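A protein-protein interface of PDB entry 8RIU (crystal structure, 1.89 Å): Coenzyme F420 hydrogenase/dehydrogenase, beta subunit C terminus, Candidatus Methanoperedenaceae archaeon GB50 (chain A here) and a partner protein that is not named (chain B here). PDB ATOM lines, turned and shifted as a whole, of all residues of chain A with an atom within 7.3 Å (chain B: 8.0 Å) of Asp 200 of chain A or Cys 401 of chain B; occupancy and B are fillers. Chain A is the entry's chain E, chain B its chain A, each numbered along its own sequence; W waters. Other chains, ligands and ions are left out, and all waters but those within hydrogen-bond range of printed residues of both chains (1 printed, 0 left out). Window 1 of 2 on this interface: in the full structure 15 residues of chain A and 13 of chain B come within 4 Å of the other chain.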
ATOM      1  N   PHE A  31      23.259 -14.068 -30.072  1.00  0.00           N
ATOM      2  CA  PHE A  31      22.655 -14.440 -28.799  1.00  0.00           C
ATOM      3  C   PHE A  31      23.571 -15.332 -27.974  1.00  0.00           C
ATOM      4  O   PHE A  31      23.118 -15.988 -27.032  1.00  0.00           O
ATOM      5  CB  PHE A  31      21.292 -15.074 -29.065  1.00  0.00           C
ATOM      6  CG  PHE A  31      20.342 -14.126 -29.731  1.00  0.00           C
ATOM      7  CD1 PHE A  31      19.652 -13.185 -28.986  1.00  0.00           C
ATOM      8  CD2 PHE A  31      20.203 -14.112 -31.111  1.00  0.00           C
ATOM      9  CE1 PHE A  31      18.803 -12.281 -29.600  1.00  0.00           C
ATOM     10  CE2 PHE A  31      19.358 -13.211 -31.725  1.00  0.00           C
ATOM     11  CZ  PHE A  31      18.660 -12.296 -30.972  1.00  0.00           C
ATOM     12  N   ASP A  58      19.678 -23.715 -31.577  1.00  0.00           N
ATOM     13  CA  ASP A  58      18.240 -23.530 -31.752  1.00  0.00           C
ATOM     14  C   ASP A  58      17.933 -22.509 -32.839  1.00  0.00           C
ATOM     15  O   ASP A  58      17.038 -22.723 -33.666  1.00  0.00           O
ATOM     16  CB  ASP A  58      17.606 -23.092 -30.436  1.00  0.00           C
ATOM     17  CG  ASP A  58      16.102 -23.026 -30.516  1.00  0.00           C
ATOM     18  OD1 ASP A  58      15.482 -24.098 -30.670  1.00  0.00           O
ATOM     19  OD2 ASP A  58      15.544 -21.908 -30.432  1.00  0.00           O
ATOM     20  N   PHE A  59      18.664 -21.394 -32.851  1.00  0.00           N
ATOM     21  CA  PHE A  59      18.384 -20.303 -33.771  1.00  0.00           C
ATOM     22  C   PHE A  59      18.998 -20.509 -35.148  1.00  0.00           C
ATOM     23  O   PHE A  59      18.642 -19.783 -36.080  1.00  0.00           O
ATOM     24  CB  PHE A  59      18.910 -18.985 -33.195  1.00  0.00           C
ATOM     25  CG  PHE A  59      18.211 -18.527 -31.943  1.00  0.00           C
ATOM     26  CD1 PHE A  59      17.033 -19.113 -31.512  1.00  0.00           C
ATOM     27  CD2 PHE A  59      18.754 -17.493 -31.187  1.00  0.00           C
ATOM     28  CE1 PHE A  59      16.404 -18.669 -30.370  1.00  0.00           C
ATOM     29  CE2 PHE A  59      18.130 -17.047 -30.048  1.00  0.00           C
ATOM     30  CZ  PHE A  59      16.953 -17.639 -29.633  1.00  0.00           C
ATOM     31  N   ILE A 193      14.037 -17.585 -34.418  1.00  0.00           N
ATOM     32  CA  ILE A 193      14.148 -16.919 -33.126  1.00  0.00           C
ATOM     33  C   ILE A 193      12.760 -16.569 -32.600  1.00  0.00           C
ATOM     34  O   ILE A 193      12.429 -16.846 -31.440  1.00  0.00           O
ATOM     35  CB  ILE A 193      15.049 -15.673 -33.246  1.00  0.00           C
ATOM     36  CG1 ILE A 193      16.488 -16.082 -33.582  1.00  0.00           C
ATOM     37  CG2 ILE A 193      15.042 -14.870 -31.960  1.00  0.00           C
ATOM     38  CD1 ILE A 193      17.306 -14.979 -34.222  1.00  0.00           C
ATOM     39  N   SER A 196      10.743 -19.833 -31.603  1.00  0.00           N
ATOM     40  CA  SER A 196      11.344 -20.797 -30.696  1.00  0.00           C
ATOM     41  C   SER A 196      10.518 -20.925 -29.425  1.00  0.00           C
ATOM     42  O   SER A 196      10.046 -19.934 -28.870  1.00  0.00           O
ATOM     43  CB  SER A 196      12.766 -20.380 -30.329  1.00  0.00           C
ATOM     44  OG  SER A 196      13.300 -21.235 -29.332  1.00  0.00           O
ATOM     45  N   LYS A 197      10.355 -22.156 -28.962  1.00  0.00           N
ATOM     46  CA  LYS A 197       9.825 -22.410 -27.632  1.00  0.00           C
ATOM     47  C   LYS A 197      10.920 -22.817 -26.657  1.00  0.00           C
ATOM     48  O   LYS A 197      10.629 -23.050 -25.480  1.00  0.00           O
ATOM     49  CB  LYS A 197       8.731 -23.482 -27.695  1.00  0.00           C
ATOM     50  CG  LYS A 197       7.362 -22.909 -28.058  1.00  0.00           C
ATOM     51  CD  LYS A 197       6.459 -23.953 -28.689  1.00  0.00           C
ATOM     52  CE  LYS A 197       4.990 -23.640 -28.457  1.00  0.00           C
ATOM     53  NZ  LYS A 197       4.723 -22.173 -28.495  1.00  0.00           N
ATOM     54  N   ALA A 198      12.173 -22.890 -27.119  1.00  0.00           N
ATOM     55  CA  ALA A 198      13.299 -23.240 -26.263  1.00  0.00           C
ATOM     56  C   ALA A 198      13.960 -22.031 -25.612  1.00  0.00           C
ATOM     57  O   ALA A 198      14.568 -22.175 -24.546  1.00  0.00           O
ATOM     58  CB  ALA A 198      14.350 -24.009 -27.073  1.00  0.00           C
ATOM     59  N   PHE A 199      13.859 -20.849 -26.223  1.00  0.00           N
ATOM     60  CA  PHE A 199      14.487 -19.646 -25.698  1.00  0.00           C
ATOM     61  C   PHE A 199      13.578 -18.451 -25.935  1.00  0.00           C
ATOM     62  O   PHE A 199      12.896 -18.366 -26.960  1.00  0.00           O
ATOM     63  CB  PHE A 199      15.858 -19.388 -26.345  1.00  0.00           C
ATOM     64  CG  PHE A 199      16.873 -20.476 -26.082  1.00  0.00           C
ATOM     65  CD1 PHE A 199      17.645 -20.463 -24.927  1.00  0.00           C
ATOM     66  CD2 PHE A 199      17.062 -21.505 -26.995  1.00  0.00           C
ATOM     67  CE1 PHE A 199      18.583 -21.464 -24.680  1.00  0.00           C
ATOM     68  CE2 PHE A 199      17.992 -22.505 -26.759  1.00  0.00           C
ATOM     69  CZ  PHE A 199      18.758 -22.485 -25.597  1.00  0.00           C
ATOM     70  N   ASP A 200      13.571 -17.536 -24.971  1.00  0.00           N
ATOM     71  CA  ASP A 200      12.892 -16.250 -25.087  1.00  0.00           C
ATOM     72  C   ASP A 200      13.958 -15.168 -24.988  1.00  0.00           C
ATOM     73  O   ASP A 200      14.477 -14.904 -23.900  1.00  0.00           O
ATOM     74  CB  ASP A 200      11.835 -16.094 -23.996  1.00  0.00           C
ATOM     75  CG  ASP A 200      11.056 -14.791 -24.105  1.00  0.00           C
ATOM     76  OD1 ASP A 200      11.371 -13.961 -24.986  1.00  0.00           O
ATOM     77  OD2 ASP A 200      10.132 -14.591 -23.286  1.00  0.00           O
ATOM     78  N   VAL A 201      14.290 -14.552 -26.117  1.00  0.00           N
ATOM     79  CA  VAL A 201      15.246 -13.456 -26.157  1.00  0.00           C
ATOM     80  C   VAL A 201      14.546 -12.136 -26.475  1.00  0.00           C
ATOM     81  O   VAL A 201      15.194 -11.166 -26.871  1.00  0.00           O
ATOM     82  CB  VAL A 201      16.383 -13.741 -27.154  1.00  0.00           C
ATOM     83  CG1 VAL A 201      17.214 -14.934 -26.701  1.00  0.00           C
ATOM     84  CG2 VAL A 201      15.826 -13.979 -28.541  1.00  0.00           C
ATOM     85  N   GLY A 202      13.224 -12.091 -26.306  1.00  0.00           N
ATOM     86  CA  GLY A 202      12.465 -10.871 -26.517  1.00  0.00           C
ATOM     87  C   GLY A 202      12.158 -10.556 -27.960  1.00  0.00           C
ATOM     88  O   GLY A 202      11.858  -9.402 -28.283  1.00  0.00           O
ATOM     89  N   ALA A 203      12.206 -11.555 -28.841  1.00  0.00           N
ATOM     90  CA  ALA A 203      12.061 -11.318 -30.271  1.00  0.00           C
ATOM     91  C   ALA A 203      10.647 -10.914 -30.666  1.00  0.00           C
ATOM     92  O   ALA A 203      10.442 -10.490 -31.807  1.00  0.00           O
ATOM     93  CB  ALA A 203      12.481 -12.567 -31.045  1.00  0.00           C
ATOM     94  N   SER A 204       9.672 -11.027 -29.768  1.00  0.00           N
ATOM     95  CA  SER A 204       8.357 -10.468 -30.062  1.00  0.00           C
ATOM     96  C   SER A 204       8.438  -8.972 -30.313  1.00  0.00           C
ATOM     97  O   SER A 204       7.521  -8.396 -30.904  1.00  0.00           O
ATOM     98  CB  SER A 204       7.400 -10.745 -28.909  1.00  0.00           C
ATOM     99  OG  SER A 204       7.868 -10.128 -27.724  1.00  0.00           O
ATOM    100  N   LYS B 395      17.465  -6.234 -11.807  1.00  0.00           N
ATOM    101  CA  LYS B 395      16.627  -6.021 -12.980  1.00  0.00           C
ATOM    102  C   LYS B 395      17.335  -6.488 -14.248  1.00  0.00           C
ATOM    103  O   LYS B 395      16.738  -7.169 -15.091  1.00  0.00           O
ATOM    104  CB  LYS B 395      16.245  -4.542 -13.065  1.00  0.00           C
ATOM    105  CG  LYS B 395      15.308  -4.166 -14.202  1.00  0.00           C
ATOM    106  CD  LYS B 395      14.950  -2.667 -14.166  1.00  0.00           C
ATOM    107  CE  LYS B 395      14.025  -2.256 -15.317  1.00  0.00           C
ATOM    108  NZ  LYS B 395      13.677  -0.798 -15.281  1.00  0.00           N
ATOM    109  N   GLU B 396      18.615  -6.138 -14.401  1.00  0.00           N
ATOM    110  CA  GLU B 396      19.344  -6.562 -15.593  1.00  0.00           C
ATOM    111  C   GLU B 396      19.418  -8.081 -15.674  1.00  0.00           C
ATOM    112  O   GLU B 396      19.350  -8.654 -16.765  1.00  0.00           O
ATOM    113  CB  GLU B 396      20.753  -5.965 -15.609  1.00  0.00           C
ATOM    114  CG  GLU B 396      20.793  -4.442 -15.681  1.00  0.00           C
ATOM    115  CD  GLU B 396      22.207  -3.885 -15.532  1.00  0.00           C
ATOM    116  OE1 GLU B 396      23.049  -4.544 -14.886  1.00  0.00           O
ATOM    117  OE2 GLU B 396      22.477  -2.788 -16.064  1.00  0.00           O
ATOM    118  N   TYR B 397      19.558  -8.748 -14.529  1.00  0.00           N
ATOM    119  CA  TYR B 397      19.711 -10.199 -14.533  1.00  0.00           C
ATOM    120  C   TYR B 397      18.432 -10.880 -14.998  1.00  0.00           C
ATOM    121  O   TYR B 397      18.463 -11.733 -15.893  1.00  0.00           O
ATOM    122  CB  TYR B 397      20.100 -10.685 -13.136  1.00  0.00           C
ATOM    123  CG  TYR B 397      21.548 -10.446 -12.761  1.00  0.00           C
ATOM    124  CD1 TYR B 397      22.575 -10.656 -13.679  1.00  0.00           C
ATOM    125  CD2 TYR B 397      21.887  -9.993 -11.492  1.00  0.00           C
ATOM    126  CE1 TYR B 397      23.891 -10.436 -13.338  1.00  0.00           C
ATOM    127  CE2 TYR B 397      23.205  -9.774 -11.140  1.00  0.00           C
ATOM    128  CZ  TYR B 397      24.203 -10.000 -12.066  1.00  0.00           C
ATOM    129  OH  TYR B 397      25.515  -9.781 -11.725  1.00  0.00           O
ATOM    130  N   VAL B 398      17.291 -10.508 -14.410  1.00  0.00           N
ATOM    131  CA  VAL B 398      16.043 -11.178 -14.758  1.00  0.00           C
ATOM    132  C   VAL B 398      15.636 -10.838 -16.181  1.00  0.00           C
ATOM    133  O   VAL B 398      14.954 -11.629 -16.846  1.00  0.00           O
ATOM    134  CB  VAL B 398      14.919 -10.818 -13.765  1.00  0.00           C
ATOM    135  CG1 VAL B 398      15.269 -11.300 -12.371  1.00  0.00           C
ATOM    136  CG2 VAL B 398      14.645  -9.320 -13.773  1.00  0.00           C
ATOM    137  N   GLU B 399      16.029  -9.663 -16.669  1.00  0.00           N
ATOM    138  CA  GLU B 399      15.680  -9.275 -18.029  1.00  0.00           C
ATOM    139  C   GLU B 399      16.538  -9.990 -19.064  1.00  0.00           C
ATOM    140  O   GLU B 399      16.051 -10.296 -20.158  1.00  0.00           O
ATOM    141  CB  GLU B 399      15.808  -7.760 -18.183  1.00  0.00           C
ATOM    142  CG  GLU B 399      14.519  -7.024 -17.852  1.00  0.00           C
ATOM    143  CD  GLU B 399      14.681  -5.515 -17.844  1.00  0.00           C
ATOM    144  OE1 GLU B 399      15.797  -5.031 -18.132  1.00  0.00           O
ATOM    145  OE2 GLU B 399      13.691  -4.810 -17.544  1.00  0.00           O
ATOM    146  N   MET B 400      17.800 -10.273 -18.738  1.00  0.00           N
ATOM    147  CA  MET B 400      18.705 -10.926 -19.674  1.00  0.00           C
ATOM    148  C   MET B 400      18.516 -12.440 -19.708  1.00  0.00           C
ATOM    149  O   MET B 400      18.956 -13.085 -20.667  1.00  0.00           O
ATOM    150  CB  MET B 400      20.152 -10.541 -19.321  1.00  0.00           C
ATOM    151  CG  MET B 400      20.806 -11.342 -18.193  1.00  0.00           C
ATOM    152  SD  MET B 400      22.605 -11.101 -18.107  1.00  0.00           S
ATOM    153  CE  MET B 400      22.694  -9.381 -17.624  1.00  0.00           C
ATOM    154  N   CYS B 401      17.862 -13.015 -18.701  1.00  0.00           N
ATOM    155  CA  CYS B 401      17.591 -14.447 -18.705  1.00  0.00           C
ATOM    156  C   CYS B 401      16.823 -14.826 -19.965  1.00  0.00           C
ATOM    157  O   CYS B 401      15.901 -14.123 -20.382  1.00  0.00           O
ATOM    158  CB  CYS B 401      16.798 -14.829 -17.455  1.00  0.00           C
ATOM    159  SG  CYS B 401      16.058 -16.478 -17.494  1.00  0.00           S
ATOM    160  N   GLN B 402      17.227 -15.931 -20.588  1.00  0.00           N
ATOM    161  CA  GLN B 402      16.623 -16.388 -21.836  1.00  0.00           C
ATOM    162  C   GLN B 402      15.492 -17.393 -21.619  1.00  0.00           C
ATOM    163  O   GLN B 402      14.972 -17.939 -22.599  1.00  0.00           O
ATOM    164  CB  GLN B 402      17.694 -17.003 -22.749  1.00  0.00           C
ATOM    165  CG  GLN B 402      18.821 -16.032 -23.151  1.00  0.00           C
ATOM    166  CD  GLN B 402      19.743 -16.583 -24.233  1.00  0.00           C
ATOM    167  OE1 GLN B 402      19.788 -17.795 -24.475  1.00  0.00           O
ATOM    168  NE2 GLN B 402      20.475 -15.688 -24.906  1.00  0.00           N
ATOM    169  N   ASN B 403      15.085 -17.632 -20.372  1.00  0.00           N
ATOM    170  CA  ASN B 403      14.000 -18.571 -20.064  1.00  0.00           C
ATOM    171  C   ASN B 403      14.248 -19.906 -20.751  1.00  0.00           C
ATOM    172  O   ASN B 403      13.372 -20.471 -21.404  1.00  0.00           O
ATOM    173  CB  ASN B 403      12.627 -18.006 -20.455  1.00  0.00           C
ATOM    174  CG  ASN B 403      11.485 -18.621 -19.642  1.00  0.00           C
ATOM    175  OD1 ASN B 403      11.719 -19.397 -18.706  1.00  0.00           O
ATOM    176  ND2 ASN B 403      10.246 -18.294 -20.007  1.00  0.00           N
ATOM    177  N   CYS B 404      15.494 -20.349 -20.658  1.00  0.00           N
ATOM    178  CA  CYS B 404      15.923 -21.608 -21.312  1.00  0.00           C
ATOM    179  C   CYS B 404      14.982 -22.756 -20.947  1.00  0.00           C
ATOM    180  O   CYS B 404      14.622 -22.883 -19.779  1.00  0.00           O
ATOM    181  CB  CYS B 404      17.358 -21.925 -20.902  1.00  0.00           C
ATOM    182  SG  CYS B 404      18.528 -20.562 -21.108  1.00  0.00           S
ATOM    183  N   ASP B 405      14.633 -23.567 -21.936  1.00  0.00           N
ATOM    184  CA  ASP B 405      13.728 -24.717 -21.711  1.00  0.00           C
ATOM    185  C   ASP B 405      14.328 -25.720 -20.730  1.00  0.00           C
ATOM    186  O   ASP B 405      13.577 -26.207 -19.896  1.00  0.00           O
ATOM    187  CB  ASP B 405      13.491 -25.461 -23.022  1.00  0.00           C
ATOM    188  CG  ASP B 405      12.048 -25.566 -23.471  1.00  0.00           C
ATOM    189  OD1 ASP B 405      11.203 -24.865 -22.903  1.00  0.00           O
ATOM    190  OD2 ASP B 405      11.794 -26.345 -24.401  1.00  0.00           O
ATOM    191  N   CYS B 408      19.278 -24.413 -16.432  1.00  0.00           N
ATOM    192  CA  CYS B 408      19.348 -24.303 -14.946  1.00  0.00           C
ATOM    193  C   CYS B 408      18.373 -25.276 -14.263  1.00  0.00           C
ATOM    194  O   CYS B 408      18.784 -25.928 -13.305  1.00  0.00           O
ATOM    195  CB  CYS B 408      19.109 -22.861 -14.502  1.00  0.00           C
ATOM    196  SG  CYS B 408      17.554 -22.137 -15.070  1.00  0.00           S
ATOM    197  N   ILE B 418      13.388 -21.593 -12.314  1.00  0.00           N
ATOM    198  CA  ILE B 418      14.172 -20.328 -12.248  1.00  0.00           C
ATOM    199  C   ILE B 418      13.851 -19.421 -13.436  1.00  0.00           C
ATOM    200  O   ILE B 418      13.629 -18.232 -13.216  1.00  0.00           O
ATOM    201  CB  ILE B 418      15.679 -20.655 -12.163  1.00  0.00           C
ATOM    202  CG1 ILE B 418      16.019 -21.415 -10.880  1.00  0.00           C
ATOM    203  CG2 ILE B 418      16.521 -19.401 -12.323  1.00  0.00           C
ATOM    204  CD1 ILE B 418      16.999 -22.544 -11.076  1.00  0.00           C
ATOM    205  N   GLY B 419      13.850 -19.973 -14.642  1.00  0.00           N
ATOM    206  CA  GLY B 419      13.643 -19.146 -15.840  1.00  0.00           C
ATOM    207  C   GLY B 419      12.296 -18.469 -15.801  1.00  0.00           C
ATOM    208  O   GLY B 419      12.231 -17.256 -15.997  1.00  0.00           O
ATOM    209  N   GLU B 420      11.271 -19.260 -15.525  1.00  0.00           N
ATOM    210  CA  GLU B 420       9.904 -18.692 -15.490  1.00  0.00           C
ATOM    211  C   GLU B 420       9.820 -17.681 -14.343  1.00  0.00           C
ATOM    212  O   GLU B 420       9.150 -16.664 -14.513  1.00  0.00           O
ATOM    213  CB  GLU B 420       8.877 -19.810 -15.353  1.00  0.00           C
ATOM    214  CG  GLU B 420       9.022 -20.901 -16.390  1.00  0.00           C
ATOM    215  CD  GLU B 420       8.457 -22.230 -15.929  1.00  0.00           C
ATOM    216  OE1 GLU B 420       7.248 -22.455 -16.113  1.00  0.00           O
ATOM    217  OE2 GLU B 420       9.226 -23.026 -15.373  1.00  0.00           O
ATOM    218  N   ALA B 421      10.497 -17.959 -13.232  1.00  0.00           N
ATOM    219  CA  ALA B 421      10.513 -17.012 -12.122  1.00  0.00           C
ATOM    220  C   ALA B 421      11.211 -15.719 -12.516  1.00  0.00           C
ATOM    221  O   ALA B 421      10.751 -14.627 -12.166  1.00  0.00           O
ATOM    222  CB  ALA B 421      11.196 -17.635 -10.904  1.00  0.00           C
ATOM    223  N   ASN B 422      12.299 -15.834 -13.261  1.00  0.00           N
ATOM    224  CA  ASN B 422      13.039 -14.628 -13.702  1.00  0.00           C
ATOM    225  C   ASN B 422      12.140 -13.777 -14.602  1.00  0.00           C
ATOM    226  O   ASN B 422      12.074 -12.568 -14.378  1.00  0.00           O
ATOM    227  CB  ASN B 422      14.344 -14.982 -14.408  1.00  0.00           C
ATOM    228  CG  ASN B 422      15.433 -15.463 -13.478  1.00  0.00           C
ATOM    229  OD1 ASN B 422      15.469 -15.086 -12.312  1.00  0.00           O
ATOM    230  ND2 ASN B 422      16.328 -16.288 -13.990  1.00  0.00           N
ATOM    231  N   LYS B 423      11.479 -14.398 -15.573  1.00  0.00           N
ATOM    232  CA  LYS B 423      10.662 -13.622 -16.540  1.00  0.00           C
ATOM    233  C   LYS B 423       9.509 -12.948 -15.788  1.00  0.00           C
ATOM    234  O   LYS B 423       9.211 -11.799 -16.095  1.00  0.00           O
ATOM    235  CB  LYS B 423      10.213 -14.533 -17.684  1.00  0.00           C
ATOM    236  CG  LYS B 423      11.331 -15.082 -18.562  1.00  0.00           C
ATOM    237  CD  LYS B 423      12.638 -14.330 -18.449  1.00  0.00           C
ATOM    238  CE  LYS B 423      12.753 -13.183 -19.430  1.00  0.00           C
ATOM    239  NZ  LYS B 423      14.043 -12.467 -19.299  1.00  0.00           N
ATOM    240  N   ALA B 426      10.995  -9.952 -14.327  1.00  0.00           N
ATOM    241  CA  ALA B 426      11.191  -8.956 -15.373  1.00  0.00           C
ATOM    242  C   ALA B 426       9.885  -8.256 -15.710  1.00  0.00           C
ATOM    243  O   ALA B 426       9.888  -7.068 -16.044  1.00  0.00           O
ATOM    244  CB  ALA B 426      11.780  -9.605 -16.626  1.00  0.00           C
ATOM    245  N   CYS B 450      24.512 -21.748 -16.703  1.00  0.00           N
ATOM    246  CA  CYS B 450      23.912 -20.502 -17.255  1.00  0.00           C
ATOM    247  C   CYS B 450      24.960 -19.700 -18.034  1.00  0.00           C
ATOM    248  O   CYS B 450      25.817 -19.091 -17.400  1.00  0.00           O
ATOM    249  CB  CYS B 450      23.285 -19.633 -16.170  1.00  0.00           C
ATOM    250  SG  CYS B 450      22.524 -18.116 -16.797  1.00  0.00           S
ATOM    251  N   LYS B 452      24.563 -16.986 -19.524  1.00  0.00           N
ATOM    252  CA  LYS B 452      24.372 -15.543 -19.235  1.00  0.00           C
ATOM    253  C   LYS B 452      25.124 -15.172 -17.951  1.00  0.00           C
ATOM    254  O   LYS B 452      25.250 -13.981 -17.699  1.00  0.00           O
ATOM    255  CB  LYS B 452      22.878 -15.221 -19.165  1.00  0.00           C
ATOM    256  CG  LYS B 452      22.073 -15.593 -20.401  1.00  0.00           C
ATOM    257  CD  LYS B 452      22.459 -14.790 -21.617  1.00  0.00           C
ATOM    258  CE  LYS B 452      22.411 -13.297 -21.379  1.00  0.00           C
ATOM    259  NZ  LYS B 452      23.037 -12.547 -22.492  1.00  0.00           N
ATOM    260  N   ILE B 454      24.285 -15.504 -14.826  1.00  0.00           N
ATOM    261  CA  ILE B 454      23.400 -14.908 -13.823  1.00  0.00           C
ATOM    262  C   ILE B 454      23.691 -15.549 -12.468  1.00  0.00           C
ATOM    263  O   ILE B 454      23.694 -16.789 -12.363  1.00  0.00           O
ATOM    264  CB  ILE B 454      21.939 -15.104 -14.224  1.00  0.00           C
ATOM    265  CG1 ILE B 454      21.649 -14.355 -15.528  1.00  0.00           C
ATOM    266  CG2 ILE B 454      21.003 -14.640 -13.121  1.00  0.00           C
ATOM    267  CD1 ILE B 454      20.227 -14.552 -16.054  1.00  0.00           C
ATOM    268  N   ILE B 456      22.238 -16.871  -9.998  1.00  0.00           N
ATOM    269  CA  ILE B 456      20.869 -17.278  -9.690  1.00  0.00           C
ATOM    270  C   ILE B 456      20.643 -17.327  -8.187  1.00  0.00           C
ATOM    271  O   ILE B 456      19.600 -16.889  -7.688  1.00  0.00           O
ATOM    272  CB  ILE B 456      20.566 -18.639 -10.353  1.00  0.00           C
ATOM    273  CG1 ILE B 456      20.525 -18.503 -11.878  1.00  0.00           C
ATOM    274  CG2 ILE B 456      19.244 -19.224  -9.855  1.00  0.00           C
ATOM    275  CD1 ILE B 456      20.759 -19.820 -12.624  1.00  0.00           C
HETATM  276  O   HOH W   1      14.014 -12.672 -22.507  1.00  0.00           O
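Printed residues of chain B within 4 Å of Phe 31 of chain A: Gln 402 (3.4 Å).
Ser 196 of chain A touches none of the printed residues of chain B.
Of the printed residues of chain B, Asp 200 of chain A touches Cys 401 (3.9 Å) and Gln 402 (2.8 Å).
Of the printed residues of chain B, Val 201 of chain A touches Gln 402.
Cys 401 of chain B touches one residue of chain A.
Printed residues of chain A within 4 Å of Asn 403 of chain B: Ala 198.
Printed residues of chain A within 4 Å of Cys 404 of chain B: Ala 198 (3.6 Å) and Phe 199 (3.7 Å).
Printed residues of chain A within 4 Å of Asp 405 of chain B: Lys 197 (3.2 Å) and Ala 198 (3.0 Å).
Of the 23 printed residues of chain B, 5 touch a printed residue of chain A.
Printed residues of chain A that touch a printed residue of chain B: Phe 31, Lys 197, Ala 198, Phe 199, Asp 200 and Val 201.
Hydrophobic or aromatic side chains of chain A within 4 Å of the printed part of chain B: Phe 199 and Val 201.
Among the printed residues, 10 pairs touch across the chains.
Among the printed residues, no Asp or Glu carboxylate lies within 4 Å of a Lys or Arg side-chain nitrogen of the other chain.
The side-chain carboxylate of Asp 405 of chain B lies close to the backbone carbonyl oxygen of Lys 197 of chain A, 3.2 Å away.
The backbone carbonyl oxygen (O) of Gln 402 of chain B is in hydrogen-bond range of the backbone NH (N) of Asp 200 of chain A (2.8 Å).
NE2 of Gln 402 of chain B lies within hydrogen-bond range of O of Phe 31 of chain A, 3.4 Å away.
O of Ala 198 of chain A is in hydrogen-bond range of N of Asp 405 of chain B (3.0 Å).
Among the printed residues, pairs that only touch across the chains: Ala 198 of chain A with Asn 403 of chain B (3.8 Å), Ala 198 of chain A with Cys 404 of chain B (3.6 Å), Phe 199 of chain A with Gln 402 of chain B (3.5 Å), Phe 199 of chain A with Cys 404 of chain B (3.7 Å), Asp 200 of chain A with Cys 401 of chain B (3.9 Å) and Val 201 of chain A with Gln 402 of chain B (3.8 Å).
Water W1 lies within hydrogen-bond range of the backbone carbonyl oxygen of Asp 200 of chain A, the backbone carbonyl oxygen of Cys 401 of chain B and the side-chain amino group of Lys 423 of chain B.
The side-chain amino group of Lys 423 of chain B lies within hydrogen-bond range of the backbone carbonyl oxygen of Cys 401 of chain B (2.7 Å).
The side-chain hydroxyl (OG) of Ser 196 of chain A is in hydrogen-bond range of the backbone NH (N) of Ala 198 of chain A (3.0 Å).
OD1 of Asp 200 of chain A lies within hydrogen-bond range of N of Gly 202 of chain A, 2.9 Å away.
The backbone NH (N) of Phe 199 of chain A is in hydrogen-bond range of the side-chain hydroxyl (OG) of Ser 196 of chain A, at 3.2 Å.
The side-chain sulfur (SG) of Cys 401 of chain B lies close to the backbone NH (N) of Asn 403 of chain B.
SG of Cys 401 of chain B sits close to ND2 of Asn 422 of chain B, 3.5 Å away.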
